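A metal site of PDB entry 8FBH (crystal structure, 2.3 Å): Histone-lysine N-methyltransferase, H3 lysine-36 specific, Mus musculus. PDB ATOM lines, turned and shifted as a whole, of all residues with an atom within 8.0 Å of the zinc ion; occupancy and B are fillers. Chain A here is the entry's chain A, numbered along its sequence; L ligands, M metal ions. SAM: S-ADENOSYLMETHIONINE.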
ATOM      1  N   ARG A 102     -24.409 -21.976  34.036  1.00  0.00           N
ATOM      2  CA  ARG A 102     -25.275 -21.528  32.916  1.00  0.00           C
ATOM      3  C   ARG A 102     -26.492 -20.810  33.484  1.00  0.00           C
ATOM      4  O   ARG A 102     -27.582 -20.882  32.867  1.00  0.00           O
ATOM      5  CB  ARG A 102     -25.681 -22.721  32.025  1.00  0.00           C
ATOM      6  CG  ARG A 102     -24.543 -23.321  31.229  1.00  0.00           C
ATOM      7  CD  ARG A 102     -24.832 -24.693  30.627  1.00  0.00           C
ATOM      8  NE  ARG A 102     -25.209 -25.632  31.683  1.00  0.00           N
ATOM      9  CZ  ARG A 102     -26.399 -26.181  31.833  1.00  0.00           C
ATOM     10  NH1 ARG A 102     -27.361 -25.966  30.941  1.00  0.00           N
ATOM     11  NH2 ARG A 102     -26.622 -26.958  32.866  1.00  0.00           N
ATOM     12  N   HIS A 171     -28.495 -23.213  25.884  1.00  0.00           N
ATOM     13  CA  HIS A 171     -27.906 -23.825  24.675  1.00  0.00           C
ATOM     14  C   HIS A 171     -27.247 -25.147  25.095  1.00  0.00           C
ATOM     15  O   HIS A 171     -26.585 -25.202  26.111  1.00  0.00           O
ATOM     16  CB  HIS A 171     -26.859 -22.923  24.027  1.00  0.00           C
ATOM     17  CG  HIS A 171     -25.969 -23.678  23.086  1.00  0.00           C
ATOM     18  ND1 HIS A 171     -26.358 -23.973  21.798  1.00  0.00           N
ATOM     19  CD2 HIS A 171     -24.772 -24.271  23.270  1.00  0.00           C
ATOM     20  CE1 HIS A 171     -25.435 -24.727  21.226  1.00  0.00           C
ATOM     21  NE2 HIS A 171     -24.456 -24.925  22.105  1.00  0.00           N
ATOM     22  N   CYS A 172     -27.339 -26.153  24.257  1.00  0.00           N
ATOM     23  CA  CYS A 172     -26.516 -27.345  24.371  1.00  0.00           C
ATOM     24  C   CYS A 172     -26.099 -27.760  22.981  1.00  0.00           C
ATOM     25  O   CYS A 172     -26.878 -27.500  22.046  1.00  0.00           O
ATOM     26  CB  CYS A 172     -27.276 -28.449  25.057  1.00  0.00           C
ATOM     27  SG  CYS A 172     -26.331 -29.965  25.052  1.00  0.00           S
ATOM     28  N   CYS A 173     -24.891 -28.343  22.864  1.00  0.00           N
ATOM     29  CA  CYS A 173     -24.364 -28.919  21.604  1.00  0.00           C
ATOM     30  C   CYS A 173     -24.890 -30.353  21.437  1.00  0.00           C
ATOM     31  O   CYS A 173     -24.844 -30.857  20.310  1.00  0.00           O
ATOM     32  CB  CYS A 173     -22.842 -28.903  21.579  1.00  0.00           C
ATOM     33  SG  CYS A 173     -22.132 -27.257  21.864  1.00  0.00           S
ATOM     34  N   GLN A 174     -25.425 -30.935  22.508  1.00  0.00           N
ATOM     35  CA  GLN A 174     -26.185 -32.224  22.474  1.00  0.00           C
ATOM     36  C   GLN A 174     -27.583 -31.998  23.032  1.00  0.00           C
ATOM     37  O   GLN A 174     -27.959 -32.488  24.088  1.00  0.00           O
ATOM     38  CB  GLN A 174     -25.432 -33.302  23.249  1.00  0.00           C
ATOM     39  CG  GLN A 174     -24.965 -34.437  22.353  1.00  0.00           C
ATOM     40  CD  GLN A 174     -24.387 -35.588  23.160  1.00  0.00           C
ATOM     41  OE1 GLN A 174     -24.185 -35.477  24.373  1.00  0.00           O
ATOM     42  NE2 GLN A 174     -24.126 -36.690  22.483  1.00  0.00           N
ATOM     43  N   ASN A 207     -30.071 -26.180  20.370  1.00  0.00           N
ATOM     44  CA  ASN A 207     -28.883 -25.609  19.703  1.00  0.00           C
ATOM     45  C   ASN A 207     -29.280 -24.200  19.322  1.00  0.00           C
ATOM     46  O   ASN A 207     -30.195 -24.081  18.502  1.00  0.00           O
ATOM     47  CB  ASN A 207     -28.454 -26.448  18.489  1.00  0.00           C
ATOM     48  CG  ASN A 207     -27.033 -26.155  18.069  1.00  0.00           C
ATOM     49  OD1 ASN A 207     -26.594 -25.003  18.030  1.00  0.00           O
ATOM     50  ND2 ASN A 207     -26.259 -27.209  17.861  1.00  0.00           N
ATOM     51  N   VAL A 219     -18.133 -18.693  25.494  1.00  0.00           N
ATOM     52  CA  VAL A 219     -17.602 -20.079  25.604  1.00  0.00           C
ATOM     53  C   VAL A 219     -18.745 -20.959  26.084  1.00  0.00           C
ATOM     54  O   VAL A 219     -19.386 -20.610  27.069  1.00  0.00           O
ATOM     55  CB  VAL A 219     -16.385 -20.178  26.546  1.00  0.00           C
ATOM     56  CG1 VAL A 219     -16.016 -21.638  26.830  1.00  0.00           C
ATOM     57  CG2 VAL A 219     -15.173 -19.395  26.007  1.00  0.00           C
ATOM     58  N   CYS A 220     -18.970 -22.071  25.406  1.00  0.00           N
ATOM     59  CA  CYS A 220     -20.049 -22.997  25.756  1.00  0.00           C
ATOM     60  C   CYS A 220     -19.618 -23.800  26.993  1.00  0.00           C
ATOM     61  O   CYS A 220     -18.479 -24.240  27.031  1.00  0.00           O
ATOM     62  CB  CYS A 220     -20.385 -23.924  24.590  1.00  0.00           C
ATOM     63  SG  CYS A 220     -21.813 -24.965  24.987  1.00  0.00           S
ATOM     64  N   LYS A 221     -20.525 -23.968  27.959  1.00  0.00           N
ATOM     65  CA  LYS A 221     -20.312 -24.804  29.163  1.00  0.00           C
ATOM     66  C   LYS A 221     -21.271 -25.990  29.156  1.00  0.00           C
ATOM     67  O   LYS A 221     -21.560 -26.448  30.232  1.00  0.00           O
ATOM     68  CB  LYS A 221     -20.547 -24.000  30.440  1.00  0.00           C
ATOM     69  CG  LYS A 221     -19.705 -22.740  30.572  1.00  0.00           C
ATOM     70  CD  LYS A 221     -18.221 -23.019  30.714  1.00  0.00           C
ATOM     71  CE  LYS A 221     -17.377 -21.772  30.846  1.00  0.00           C
ATOM     72  NZ  LYS A 221     -15.933 -22.090  30.919  1.00  0.00           N
ATOM     73  N   CYS A 222     -21.777 -26.431  27.998  1.00  0.00           N
ATOM     74  CA  CYS A 222     -22.828 -27.484  27.949  1.00  0.00           C
ATOM     75  C   CYS A 222     -22.248 -28.804  28.470  1.00  0.00           C
ATOM     76  O   CYS A 222     -23.036 -29.593  29.000  1.00  0.00           O
ATOM     77  CB  CYS A 222     -23.462 -27.657  26.568  1.00  0.00           C
ATOM     78  SG  CYS A 222     -22.438 -28.479  25.318  1.00  0.00           S
ATOM     79  N   GLY A 223     -20.934 -29.018  28.360  1.00  0.00           N
ATOM     80  CA  GLY A 223     -20.213 -30.193  28.906  1.00  0.00           C
ATOM     81  C   GLY A 223     -20.449 -31.474  28.096  1.00  0.00           C
ATOM     82  O   GLY A 223     -20.210 -32.558  28.638  1.00  0.00           O
ATOM     83  N   ALA A 224     -20.875 -31.375  26.834  1.00  0.00           N
ATOM     84  CA  ALA A 224     -21.109 -32.547  25.958  1.00  0.00           C
ATOM     85  C   ALA A 224     -19.777 -33.000  25.342  1.00  0.00           C
ATOM     86  O   ALA A 224     -18.868 -32.193  25.159  1.00  0.00           O
ATOM     87  CB  ALA A 224     -22.134 -32.221  24.905  1.00  0.00           C
ATOM     88  N   PRO A 225     -19.612 -34.311  25.020  1.00  0.00           N
ATOM     89  CA  PRO A 225     -18.383 -34.783  24.379  1.00  0.00           C
ATOM     90  C   PRO A 225     -18.051 -34.049  23.062  1.00  0.00           C
ATOM     91  O   PRO A 225     -16.893 -33.745  22.863  1.00  0.00           O
ATOM     92  CB  PRO A 225     -18.608 -36.293  24.147  1.00  0.00           C
ATOM     93  CG  PRO A 225     -20.076 -36.568  24.500  1.00  0.00           C
ATOM     94  CD  PRO A 225     -20.541 -35.396  25.356  1.00  0.00           C
ATOM     95  N   ASN A 226     -19.066 -33.693  22.257  1.00  0.00           N
ATOM     96  CA  ASN A 226     -18.905 -33.078  20.907  1.00  0.00           C
ATOM     97  C   ASN A 226     -19.110 -31.537  20.957  1.00  0.00           C
ATOM     98  O   ASN A 226     -19.428 -30.947  19.923  1.00  0.00           O
ATOM     99  CB  ASN A 226     -19.850 -33.756  19.906  1.00  0.00           C
ATOM    100  CG  ASN A 226     -21.303 -33.732  20.336  1.00  0.00           C
ATOM    101  OD1 ASN A 226     -21.621 -33.990  21.501  1.00  0.00           O
ATOM    102  ND2 ASN A 226     -22.197 -33.450  19.397  1.00  0.00           N
ATOM    103  N   CYS A 227     -18.933 -30.900  22.115  1.00  0.00           N
ATOM    104  CA  CYS A 227     -19.150 -29.436  22.314  1.00  0.00           C
ATOM    105  C   CYS A 227     -18.290 -28.667  21.310  1.00  0.00           C
ATOM    106  O   CYS A 227     -17.086 -28.939  21.234  1.00  0.00           O
ATOM    107  CB  CYS A 227     -18.816 -29.031  23.749  1.00  0.00           C
ATOM    108  SG  CYS A 227     -18.966 -27.264  24.097  1.00  0.00           S
ATOM    109  N   SER A 228     -18.897 -27.737  20.574  1.00  0.00           N
ATOM    110  CA  SER A 228     -18.215 -26.861  19.572  1.00  0.00           C
ATOM    111  C   SER A 228     -17.295 -25.836  20.262  1.00  0.00           C
ATOM    112  O   SER A 228     -16.497 -25.205  19.556  1.00  0.00           O
ATOM    113  CB  SER A 228     -19.242 -26.164  18.734  1.00  0.00           C
ATOM    114  OG  SER A 228     -19.981 -25.252  19.556  1.00  0.00           O
ATOM    115  N   GLY A 229     -17.490 -25.598  21.565  1.00  0.00           N
ATOM    116  CA  GLY A 229     -16.864 -24.467  22.292  1.00  0.00           C
ATOM    117  C   GLY A 229     -17.686 -23.163  22.271  1.00  0.00           C
ATOM    118  O   GLY A 229     -17.335 -22.252  23.040  1.00  0.00           O
ATOM    119  N   PHE A 230     -18.742 -23.068  21.455  1.00  0.00           N
ATOM    120  CA  PHE A 230     -19.529 -21.833  21.240  1.00  0.00           C
ATOM    121  C   PHE A 230     -21.044 -22.132  21.248  1.00  0.00           C
ATOM    122  O   PHE A 230     -21.465 -23.330  21.227  1.00  0.00           O
ATOM    123  CB  PHE A 230     -19.065 -21.133  19.964  1.00  0.00           C
ATOM    124  CG  PHE A 230     -19.003 -21.951  18.693  1.00  0.00           C
ATOM    125  CD1 PHE A 230     -20.142 -22.167  17.913  1.00  0.00           C
ATOM    126  CD2 PHE A 230     -17.782 -22.414  18.208  1.00  0.00           C
ATOM    127  CE1 PHE A 230     -20.053 -22.840  16.693  1.00  0.00           C
ATOM    128  CE2 PHE A 230     -17.693 -23.088  16.988  1.00  0.00           C
ATOM    129  CZ  PHE A 230     -18.838 -23.305  16.227  1.00  0.00           C
ATOM    130  N   LEU A 231     -21.869 -21.087  21.323  1.00  0.00           N
ATOM    131  CA  LEU A 231     -23.350 -21.264  21.435  1.00  0.00           C
ATOM    132  C   LEU A 231     -23.910 -21.548  20.029  1.00  0.00           C
ATOM    133  O   LEU A 231     -24.825 -20.805  19.557  1.00  0.00           O
ATOM    134  CB  LEU A 231     -23.966 -20.041  22.119  1.00  0.00           C
ATOM    135  CG  LEU A 231     -23.490 -19.754  23.551  1.00  0.00           C
ATOM    136  CD1 LEU A 231     -24.542 -18.986  24.345  1.00  0.00           C
ATOM    137  CD2 LEU A 231     -23.124 -21.021  24.291  1.00  0.00           C
ATOM    138  N   GLY A 232     -23.361 -22.588  19.367  1.00  0.00           N
ATOM    139  CA  GLY A 232     -23.779 -23.005  18.008  1.00  0.00           C
ATOM    140  C   GLY A 232     -23.183 -24.338  17.553  1.00  0.00           C
ATOM    141  O   GLY A 232     -22.450 -25.045  18.262  1.00  0.00           O
ATOM    142  OXT GLY A 232     -23.453 -24.736  16.392  1.00  0.00           O
HETATM  143  N   SAM L   1     -29.376 -19.149  31.669  1.00  0.00           N
HETATM  144  CA  SAM L   1     -30.263 -18.027  31.275  1.00  0.00           C
HETATM  145  C   SAM L   1     -30.736 -17.259  32.534  1.00  0.00           C
HETATM  146  O   SAM L   1     -30.093 -17.448  33.608  1.00  0.00           O
HETATM  147  OXT SAM L   1     -31.709 -16.491  32.404  1.00  0.00           O
HETATM  148  CB  SAM L   1     -31.441 -18.583  30.480  1.00  0.00           C
HETATM  149  CG  SAM L   1     -31.119 -18.778  28.990  1.00  0.00           C
HETATM  150  SD  SAM L   1     -30.932 -17.156  28.183  1.00  0.00           S
HETATM  151  CE  SAM L   1     -32.064 -17.318  26.807  1.00  0.00           C
HETATM  152  C5' SAM L   1     -29.349 -17.337  27.330  1.00  0.00           C
HETATM  153  C4' SAM L   1     -28.128 -16.991  28.157  1.00  0.00           C
HETATM  154  O4' SAM L   1     -27.802 -18.103  29.031  1.00  0.00           O
HETATM  155  C3' SAM L   1     -26.870 -16.736  27.344  1.00  0.00           C
HETATM  156  O3' SAM L   1     -26.822 -15.378  26.926  1.00  0.00           O
HETATM  157  C2' SAM L   1     -25.770 -17.136  28.332  1.00  0.00           C
HETATM  158  O2' SAM L   1     -25.457 -16.113  29.245  1.00  0.00           O
HETATM  159  C1' SAM L   1     -26.401 -18.325  29.065  1.00  0.00           C
HETATM  160  N9  SAM L   1     -26.136 -19.636  28.470  1.00  0.00           N
HETATM  161  C8  SAM L   1     -27.066 -20.460  27.896  1.00  0.00           C
HETATM  162  N7  SAM L   1     -26.570 -21.599  27.474  1.00  0.00           N
HETATM  163  C5  SAM L   1     -25.213 -21.528  27.788  1.00  0.00           C
HETATM  164  C6  SAM L   1     -24.148 -22.433  27.601  1.00  0.00           C
HETATM  165  N6  SAM L   1     -24.276 -23.629  27.043  1.00  0.00           N
HETATM  166  N1  SAM L   1     -22.926 -22.046  28.009  1.00  0.00           N
HETATM  167  C2  SAM L   1     -22.799 -20.843  28.588  1.00  0.00           C
HETATM  168  N3  SAM L   1     -23.728 -19.938  28.862  1.00  0.00           N
HETATM  169  C4  SAM L   1     -24.936 -20.336  28.416  1.00  0.00           C
HETATM  170 ZN    ZN M   1     -21.376 -26.914  24.004  1.00  0.00          ZN
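SG of Cys 220 binds the zinc ion (2.2 Å).
SG of Cys 173 binds the zinc ion (2.3 Å).
SG of Cys 222 binds the zinc ion, 2.3 Å away.
SG of Cys 227 binds the zinc ion (2.4 Å).
The zinc ion has four donor atoms within binding distance.
N of Cys 220 is in hydrogen-bond range of O of Gly 229 (2.9 Å).
NE2 of His 171 sits close to SG of Cys 173, at 3.3 Å.
N of Ser 228 lies close to SG of Cys 173 (3.5 Å).
The backbone NH (N) of Ala 224 lies close to the side-chain sulfur (SG) of Cys 222 (3.6 Å).
SG of Cys 227 lies close to N of Gly 229 (3.4 Å).
Within 4 Å of the zinc ion: Cys 173, Cys 220, Cys 222 and Cys 227.
SG of Cys 220 lies close to N6 of the ligand (3.5 Å).
The backbone NH of His 171 sits at hydrogen-bond distance from a nitrogen (N7) of the ligand (3.0 Å).
The backbone carbonyl oxygen of His 171 sits at hydrogen-bond distance from a nitrogen (N6) of the ligand (2.9 Å).
N of Lys 221 is in hydrogen-bond range of N1 of the ligand (3.1 Å).
The backbone carbonyl oxygen of Arg 102 is in hydrogen-bond range of a nitrogen (N) of the ligand (2.8 Å).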
